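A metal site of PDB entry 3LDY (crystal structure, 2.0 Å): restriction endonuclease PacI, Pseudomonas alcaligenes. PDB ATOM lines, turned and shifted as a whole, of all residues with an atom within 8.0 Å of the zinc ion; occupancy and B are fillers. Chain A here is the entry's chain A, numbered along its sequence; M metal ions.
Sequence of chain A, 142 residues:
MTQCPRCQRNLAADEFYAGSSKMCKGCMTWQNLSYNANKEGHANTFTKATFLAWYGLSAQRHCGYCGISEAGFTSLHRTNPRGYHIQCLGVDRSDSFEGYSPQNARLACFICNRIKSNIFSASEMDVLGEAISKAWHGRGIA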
ATOM      1  N   GLN A   3      27.116  -8.399 -17.318  1.00  0.00           N
ATOM      2  CA  GLN A   3      26.519  -9.676 -16.936  1.00  0.00           C
ATOM      3  C   GLN A   3      26.357  -9.866 -15.439  1.00  0.00           C
ATOM      4  O   GLN A   3      27.278  -9.622 -14.661  1.00  0.00           O
ATOM      5  CB  GLN A   3      27.353 -10.829 -17.500  1.00  0.00           C
ATOM      6  CG  GLN A   3      26.645 -12.164 -17.426  1.00  0.00           C
ATOM      7  CD  GLN A   3      27.461 -13.279 -18.025  1.00  0.00           C
ATOM      8  OE1 GLN A   3      28.583 -13.551 -17.589  1.00  0.00           O
ATOM      9  NE2 GLN A   3      26.903 -13.947 -19.034  1.00  0.00           N
ATOM     10  N   CYS A   4      25.169 -10.328 -15.046  1.00  0.00           N
ATOM     11  CA  CYS A   4      24.919 -10.578 -13.632  1.00  0.00           C
ATOM     12  C   CYS A   4      25.538 -11.919 -13.244  1.00  0.00           C
ATOM     13  O   CYS A   4      25.248 -12.926 -13.877  1.00  0.00           O
ATOM     14  CB  CYS A   4      23.403 -10.552 -13.326  1.00  0.00           C
ATOM     15  SG  CYS A   4      22.953 -11.147 -11.678  1.00  0.00           S
ATOM     16  N   PRO A   5      26.397 -11.921 -12.204  1.00  0.00           N
ATOM     17  CA  PRO A   5      27.090 -13.173 -11.855  1.00  0.00           C
ATOM     18  C   PRO A   5      26.132 -14.264 -11.365  1.00  0.00           C
ATOM     19  O   PRO A   5      26.531 -15.419 -11.208  1.00  0.00           O
ATOM     20  CB  PRO A   5      28.039 -12.738 -10.719  1.00  0.00           C
ATOM     21  CG  PRO A   5      27.383 -11.550 -10.115  1.00  0.00           C
ATOM     22  CD  PRO A   5      26.727 -10.829 -11.266  1.00  0.00           C
ATOM     23  N   ARG A   6      24.870 -13.898 -11.143  1.00  0.00           N
ATOM     24  CA  ARG A   6      23.882 -14.823 -10.599  1.00  0.00           C
ATOM     25  C   ARG A   6      22.930 -15.392 -11.655  1.00  0.00           C
ATOM     26  O   ARG A   6      22.924 -16.593 -11.873  1.00  0.00           O
ATOM     27  CB  ARG A   6      23.090 -14.184  -9.452  1.00  0.00           C
ATOM     28  CG  ARG A   6      22.042 -15.114  -8.870  1.00  0.00           C
ATOM     29  CD  ARG A   6      22.549 -15.911  -7.689  1.00  0.00           C
ATOM     30  NE  ARG A   6      22.566 -15.079  -6.489  1.00  0.00           N
ATOM     31  CZ  ARG A   6      22.438 -15.538  -5.249  1.00  0.00           C
ATOM     32  NH1 ARG A   6      22.284 -16.851  -5.026  1.00  0.00           N
ATOM     33  NH2 ARG A   6      22.457 -14.692  -4.230  1.00  0.00           N
ATOM     34  N   CYS A   7      22.124 -14.558 -12.299  1.00  0.00           N
ATOM     35  CA  CYS A   7      21.240 -15.055 -13.370  1.00  0.00           C
ATOM     36  C   CYS A   7      21.959 -15.166 -14.714  1.00  0.00           C
ATOM     37  O   CYS A   7      21.398 -15.692 -15.667  1.00  0.00           O
ATOM     38  CB  CYS A   7      20.005 -14.169 -13.527  1.00  0.00           C
ATOM     39  SG  CYS A   7      20.397 -12.458 -14.029  1.00  0.00           S
ATOM     40  N   GLN A   8      23.188 -14.629 -14.781  1.00  0.00           N
ATOM     41  CA  GLN A   8      23.995 -14.514 -15.987  1.00  0.00           C
ATOM     42  C   GLN A   8      23.342 -13.756 -17.148  1.00  0.00           C
ATOM     43  O   GLN A   8      23.823 -13.820 -18.289  1.00  0.00           O
ATOM     44  CB  GLN A   8      24.546 -15.877 -16.442  1.00  0.00           C
ATOM     45  CG  GLN A   8      25.855 -16.230 -15.760  1.00  0.00           C
ATOM     46  CD  GLN A   8      25.758 -17.555 -15.021  1.00  0.00           C
ATOM     47  OE1 GLN A   8      24.970 -17.691 -14.082  1.00  0.00           O
ATOM     48  NE2 GLN A   8      26.559 -18.533 -15.446  1.00  0.00           N
ATOM     49  N   ARG A   9      22.276 -13.015 -16.852  1.00  0.00           N
ATOM     50  CA  ARG A   9      21.686 -12.196 -17.905  1.00  0.00           C
ATOM     51  C   ARG A   9      22.585 -11.018 -18.261  1.00  0.00           C
ATOM     52  O   ARG A   9      23.361 -10.524 -17.415  1.00  0.00           O
ATOM     53  CB  ARG A   9      20.297 -11.703 -17.532  1.00  0.00           C
ATOM     54  CG  ARG A   9      19.216 -12.778 -17.567  1.00  0.00           C
ATOM     55  CD  ARG A   9      17.889 -12.177 -17.132  1.00  0.00           C
ATOM     56  NE  ARG A   9      17.974 -11.512 -15.820  1.00  0.00           N
ATOM     57  CZ  ARG A   9      17.087 -10.637 -15.353  1.00  0.00           C
ATOM     58  NH1 ARG A   9      16.022 -10.273 -16.077  1.00  0.00           N
ATOM     59  NH2 ARG A   9      17.270 -10.102 -14.150  1.00  0.00           N
ATOM     60  N   ASN A  10      22.480 -10.592 -19.517  1.00  0.00           N
ATOM     61  CA  ASN A  10      23.114  -9.351 -19.961  1.00  0.00           C
ATOM     62  C   ASN A  10      22.256  -8.109 -19.858  1.00  0.00           C
ATOM     63  O   ASN A  10      21.254  -7.944 -20.581  1.00  0.00           O
ATOM     64  CB  ASN A  10      23.720  -9.490 -21.356  1.00  0.00           C
ATOM     65  CG  ASN A  10      25.205  -9.443 -21.331  1.00  0.00           C
ATOM     66  OD1 ASN A  10      25.869 -10.491 -21.326  1.00  0.00           O
ATOM     67  ND2 ASN A  10      25.763  -8.227 -21.265  1.00  0.00           N
ATOM     68  N   LEU A  11      22.661  -7.208 -18.958  1.00  0.00           N
ATOM     69  CA  LEU A  11      21.770  -6.180 -18.442  1.00  0.00           C
ATOM     70  C   LEU A  11      22.375  -4.788 -18.516  1.00  0.00           C
ATOM     71  O   LEU A  11      23.596  -4.632 -18.437  1.00  0.00           O
ATOM     72  CB  LEU A  11      21.391  -6.525 -17.000  1.00  0.00           C
ATOM     73  CG  LEU A  11      20.592  -7.809 -16.769  1.00  0.00           C
ATOM     74  CD1 LEU A  11      20.590  -8.234 -15.330  1.00  0.00           C
ATOM     75  CD2 LEU A  11      19.168  -7.674 -17.290  1.00  0.00           C
ATOM     76  N   GLU A  15      19.812  -1.978 -14.104  1.00  0.00           N
ATOM     77  CA  GLU A  15      19.352  -3.235 -13.480  1.00  0.00           C
ATOM     78  C   GLU A  15      20.249  -3.609 -12.318  1.00  0.00           C
ATOM     79  O   GLU A  15      19.968  -4.600 -11.617  1.00  0.00           O
ATOM     80  CB  GLU A  15      19.419  -4.404 -14.452  1.00  0.00           C
ATOM     81  CG  GLU A  15      18.150  -4.797 -15.184  1.00  0.00           C
ATOM     82  CD  GLU A  15      16.832  -4.512 -14.495  1.00  0.00           C
ATOM     83  OE1 GLU A  15      16.447  -5.157 -13.495  1.00  0.00           O
ATOM     84  OE2 GLU A  15      16.148  -3.628 -15.019  1.00  0.00           O
ATOM     85  N   PHE A  16      21.330  -2.855 -12.149  1.00  0.00           N
ATOM     86  CA  PHE A  16      22.265  -3.082 -11.045  1.00  0.00           C
ATOM     87  C   PHE A  16      22.155  -2.000  -9.953  1.00  0.00           C
ATOM     88  O   PHE A  16      21.543  -0.948 -10.160  1.00  0.00           O
ATOM     89  CB  PHE A  16      23.705  -3.246 -11.610  1.00  0.00           C
ATOM     90  CG  PHE A  16      23.866  -4.506 -12.456  1.00  0.00           C
ATOM     91  CD1 PHE A  16      23.874  -4.426 -13.849  1.00  0.00           C
ATOM     92  CD2 PHE A  16      23.953  -5.769 -11.853  1.00  0.00           C
ATOM     93  CE1 PHE A  16      23.996  -5.592 -14.636  1.00  0.00           C
ATOM     94  CE2 PHE A  16      24.059  -6.943 -12.616  1.00  0.00           C
ATOM     95  CZ  PHE A  16      24.084  -6.854 -14.019  1.00  0.00           C
ATOM     96  N   LYS A  22      26.845  -6.974  -6.068  1.00  0.00           N
ATOM     97  CA  LYS A  22      27.172  -7.332  -7.439  1.00  0.00           C
ATOM     98  C   LYS A  22      25.999  -7.932  -8.255  1.00  0.00           C
ATOM     99  O   LYS A  22      25.976  -7.772  -9.481  1.00  0.00           O
ATOM    100  CB  LYS A  22      28.396  -8.249  -7.465  1.00  0.00           C
ATOM    101  CG  LYS A  22      29.733  -7.558  -7.121  1.00  0.00           C
ATOM    102  CD  LYS A  22      30.908  -8.556  -7.220  1.00  0.00           C
ATOM    103  CE  LYS A  22      32.244  -7.934  -6.814  1.00  0.00           C
ATOM    104  NZ  LYS A  22      33.360  -8.926  -6.882  1.00  0.00           N
ATOM    105  N   MET A  23      25.043  -8.596  -7.588  1.00  0.00           N
ATOM    106  CA  MET A  23      23.910  -9.197  -8.303  1.00  0.00           C
ATOM    107  C   MET A  23      22.888  -8.136  -8.779  1.00  0.00           C
ATOM    108  O   MET A  23      22.804  -7.062  -8.187  1.00  0.00           O
ATOM    109  CB  MET A  23      23.237 -10.301  -7.458  1.00  0.00           C
ATOM    110  CG  MET A  23      22.330  -9.809  -6.333  1.00  0.00           C
ATOM    111  SD  MET A  23      21.584 -11.172  -5.396  1.00  0.00           S
ATOM    112  CE  MET A  23      22.753 -11.312  -4.021  1.00  0.00           C
ATOM    113  N   CYS A  24      22.126  -8.450  -9.824  1.00  0.00           N
ATOM    114  CA  CYS A  24      21.108  -7.543 -10.350  1.00  0.00           C
ATOM    115  C   CYS A  24      19.877  -7.359  -9.426  1.00  0.00           C
ATOM    116  O   CYS A  24      19.670  -8.129  -8.485  1.00  0.00           O
ATOM    117  CB  CYS A  24      20.663  -7.957 -11.759  1.00  0.00           C
ATOM    118  SG  CYS A  24      19.503  -9.342 -11.828  1.00  0.00           S
ATOM    119  N   LYS A  25      19.060  -6.354  -9.718  1.00  0.00           N
ATOM    120  CA  LYS A  25      17.867  -6.048  -8.901  1.00  0.00           C
ATOM    121  C   LYS A  25      16.854  -7.202  -8.872  1.00  0.00           C
ATOM    122  O   LYS A  25      16.234  -7.450  -7.847  1.00  0.00           O
ATOM    123  CB  LYS A  25      17.178  -4.775  -9.396  1.00  0.00           C
ATOM    124  CG  LYS A  25      17.974  -3.493  -9.202  1.00  0.00           C
ATOM    125  CD  LYS A  25      17.317  -2.350  -9.960  1.00  0.00           C
ATOM    126  CE  LYS A  25      17.980  -1.008  -9.624  1.00  0.00           C
ATOM    127  NZ  LYS A  25      17.267   0.120 -10.308  1.00  0.00           N
ATOM    128  N   GLY A  26      16.700  -7.877 -10.014  1.00  0.00           N
ATOM    129  CA  GLY A  26      15.818  -9.045 -10.121  1.00  0.00           C
ATOM    130  C   GLY A  26      16.285 -10.174  -9.231  1.00  0.00           C
ATOM    131  O   GLY A  26      15.488 -10.757  -8.459  1.00  0.00           O
ATOM    132  N   CYS A  27      17.581 -10.490  -9.325  1.00  0.00           N
ATOM    133  CA  CYS A  27      18.174 -11.507  -8.462  1.00  0.00           C
ATOM    134  C   CYS A  27      18.030 -11.146  -6.986  1.00  0.00           C
ATOM    135  O   CYS A  27      17.575 -11.962  -6.180  1.00  0.00           O
ATOM    136  CB  CYS A  27      19.658 -11.770  -8.843  1.00  0.00           C
ATOM    137  SG  CYS A  27      19.843 -12.852 -10.307  1.00  0.00           S
ATOM    138  N   MET A  28      18.371  -9.913  -6.633  1.00  0.00           N
ATOM    139  CA  MET A  28      18.273  -9.475  -5.240  1.00  0.00           C
ATOM    140  C   MET A  28      16.835  -9.499  -4.701  1.00  0.00           C
ATOM    141  O   MET A  28      16.587  -9.908  -3.558  1.00  0.00           O
ATOM    142  CB  MET A  28      18.881  -8.088  -5.071  1.00  0.00           C
ATOM    143  CG  MET A  28      18.846  -7.571  -3.622  1.00  0.00           C
ATOM    144  SD  MET A  28      19.968  -8.469  -2.532  1.00  0.00           S
ATOM    145  CE  MET A  28      21.382  -7.385  -2.611  1.00  0.00           C
ATOM    146  N   LYS A  48      12.022 -18.826 -10.040  1.00  0.00           N
ATOM    147  CA  LYS A  48      12.920 -17.706 -10.343  1.00  0.00           C
ATOM    148  C   LYS A  48      12.661 -17.185 -11.772  1.00  0.00           C
ATOM    149  O   LYS A  48      12.506 -15.979 -11.973  1.00  0.00           O
ATOM    150  CB  LYS A  48      14.405 -18.073 -10.171  1.00  0.00           C
ATOM    151  CG  LYS A  48      15.299 -16.839 -10.092  1.00  0.00           C
ATOM    152  CD  LYS A  48      16.789 -17.183  -9.987  1.00  0.00           C
ATOM    153  CE  LYS A  48      17.520 -16.004  -9.395  1.00  0.00           C
ATOM    154  NZ  LYS A  48      18.989 -15.995  -9.616  1.00  0.00           N
ATOM    155  N   LEU A  52      11.488 -13.483 -12.768  1.00  0.00           N
ATOM    156  CA  LEU A  52      12.346 -12.595 -13.539  1.00  0.00           C
ATOM    157  C   LEU A  52      11.617 -12.059 -14.768  1.00  0.00           C
ATOM    158  O   LEU A  52      11.775 -10.895 -15.084  1.00  0.00           O
ATOM    159  CB  LEU A  52      13.667 -13.254 -13.948  1.00  0.00           C
ATOM    160  CG  LEU A  52      14.706 -13.597 -12.855  1.00  0.00           C
ATOM    161  CD1 LEU A  52      15.984 -14.142 -13.501  1.00  0.00           C
ATOM    162  CD2 LEU A  52      15.033 -12.440 -11.885  1.00  0.00           C
HETATM  163 ZN    ZN M   1      20.662 -11.408 -11.900  1.00  0.00          ZN
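Of the 20 residues printed, 4 come within 4 Å of the zinc ion.
SG of Cys 27 sits close to NZ of Lys 48 (3.3 Å).
N of Cys 4 is in hydrogen-bond range of O of Arg 9 (3.0 Å).
SG of Cys 4 lies close to N of Arg 6 (3.4 Å).
The side-chain sulfur of Cys 24 lies close to the guanidinium group of Arg 9.
The backbone NH (N) of Gly 26 lies close to the side-chain sulfur (SG) of Cys 24.
The guanidinium group (NE) of Arg 9 lies close to the side-chain sulfur (SG) of Cys 7 (3.2 Å).
SG of Cys 27 is bound to the zinc ion (2.3 Å).
The side-chain sulfur (SG) of Cys 4 is bound to the zinc ion (2.3 Å).
SG of Cys 24 is bound to the zinc ion (2.4 Å).
The zinc ion is bound by SG of Cys 7 (2.4 Å).
The zinc ion has four donor atoms within binding distance.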
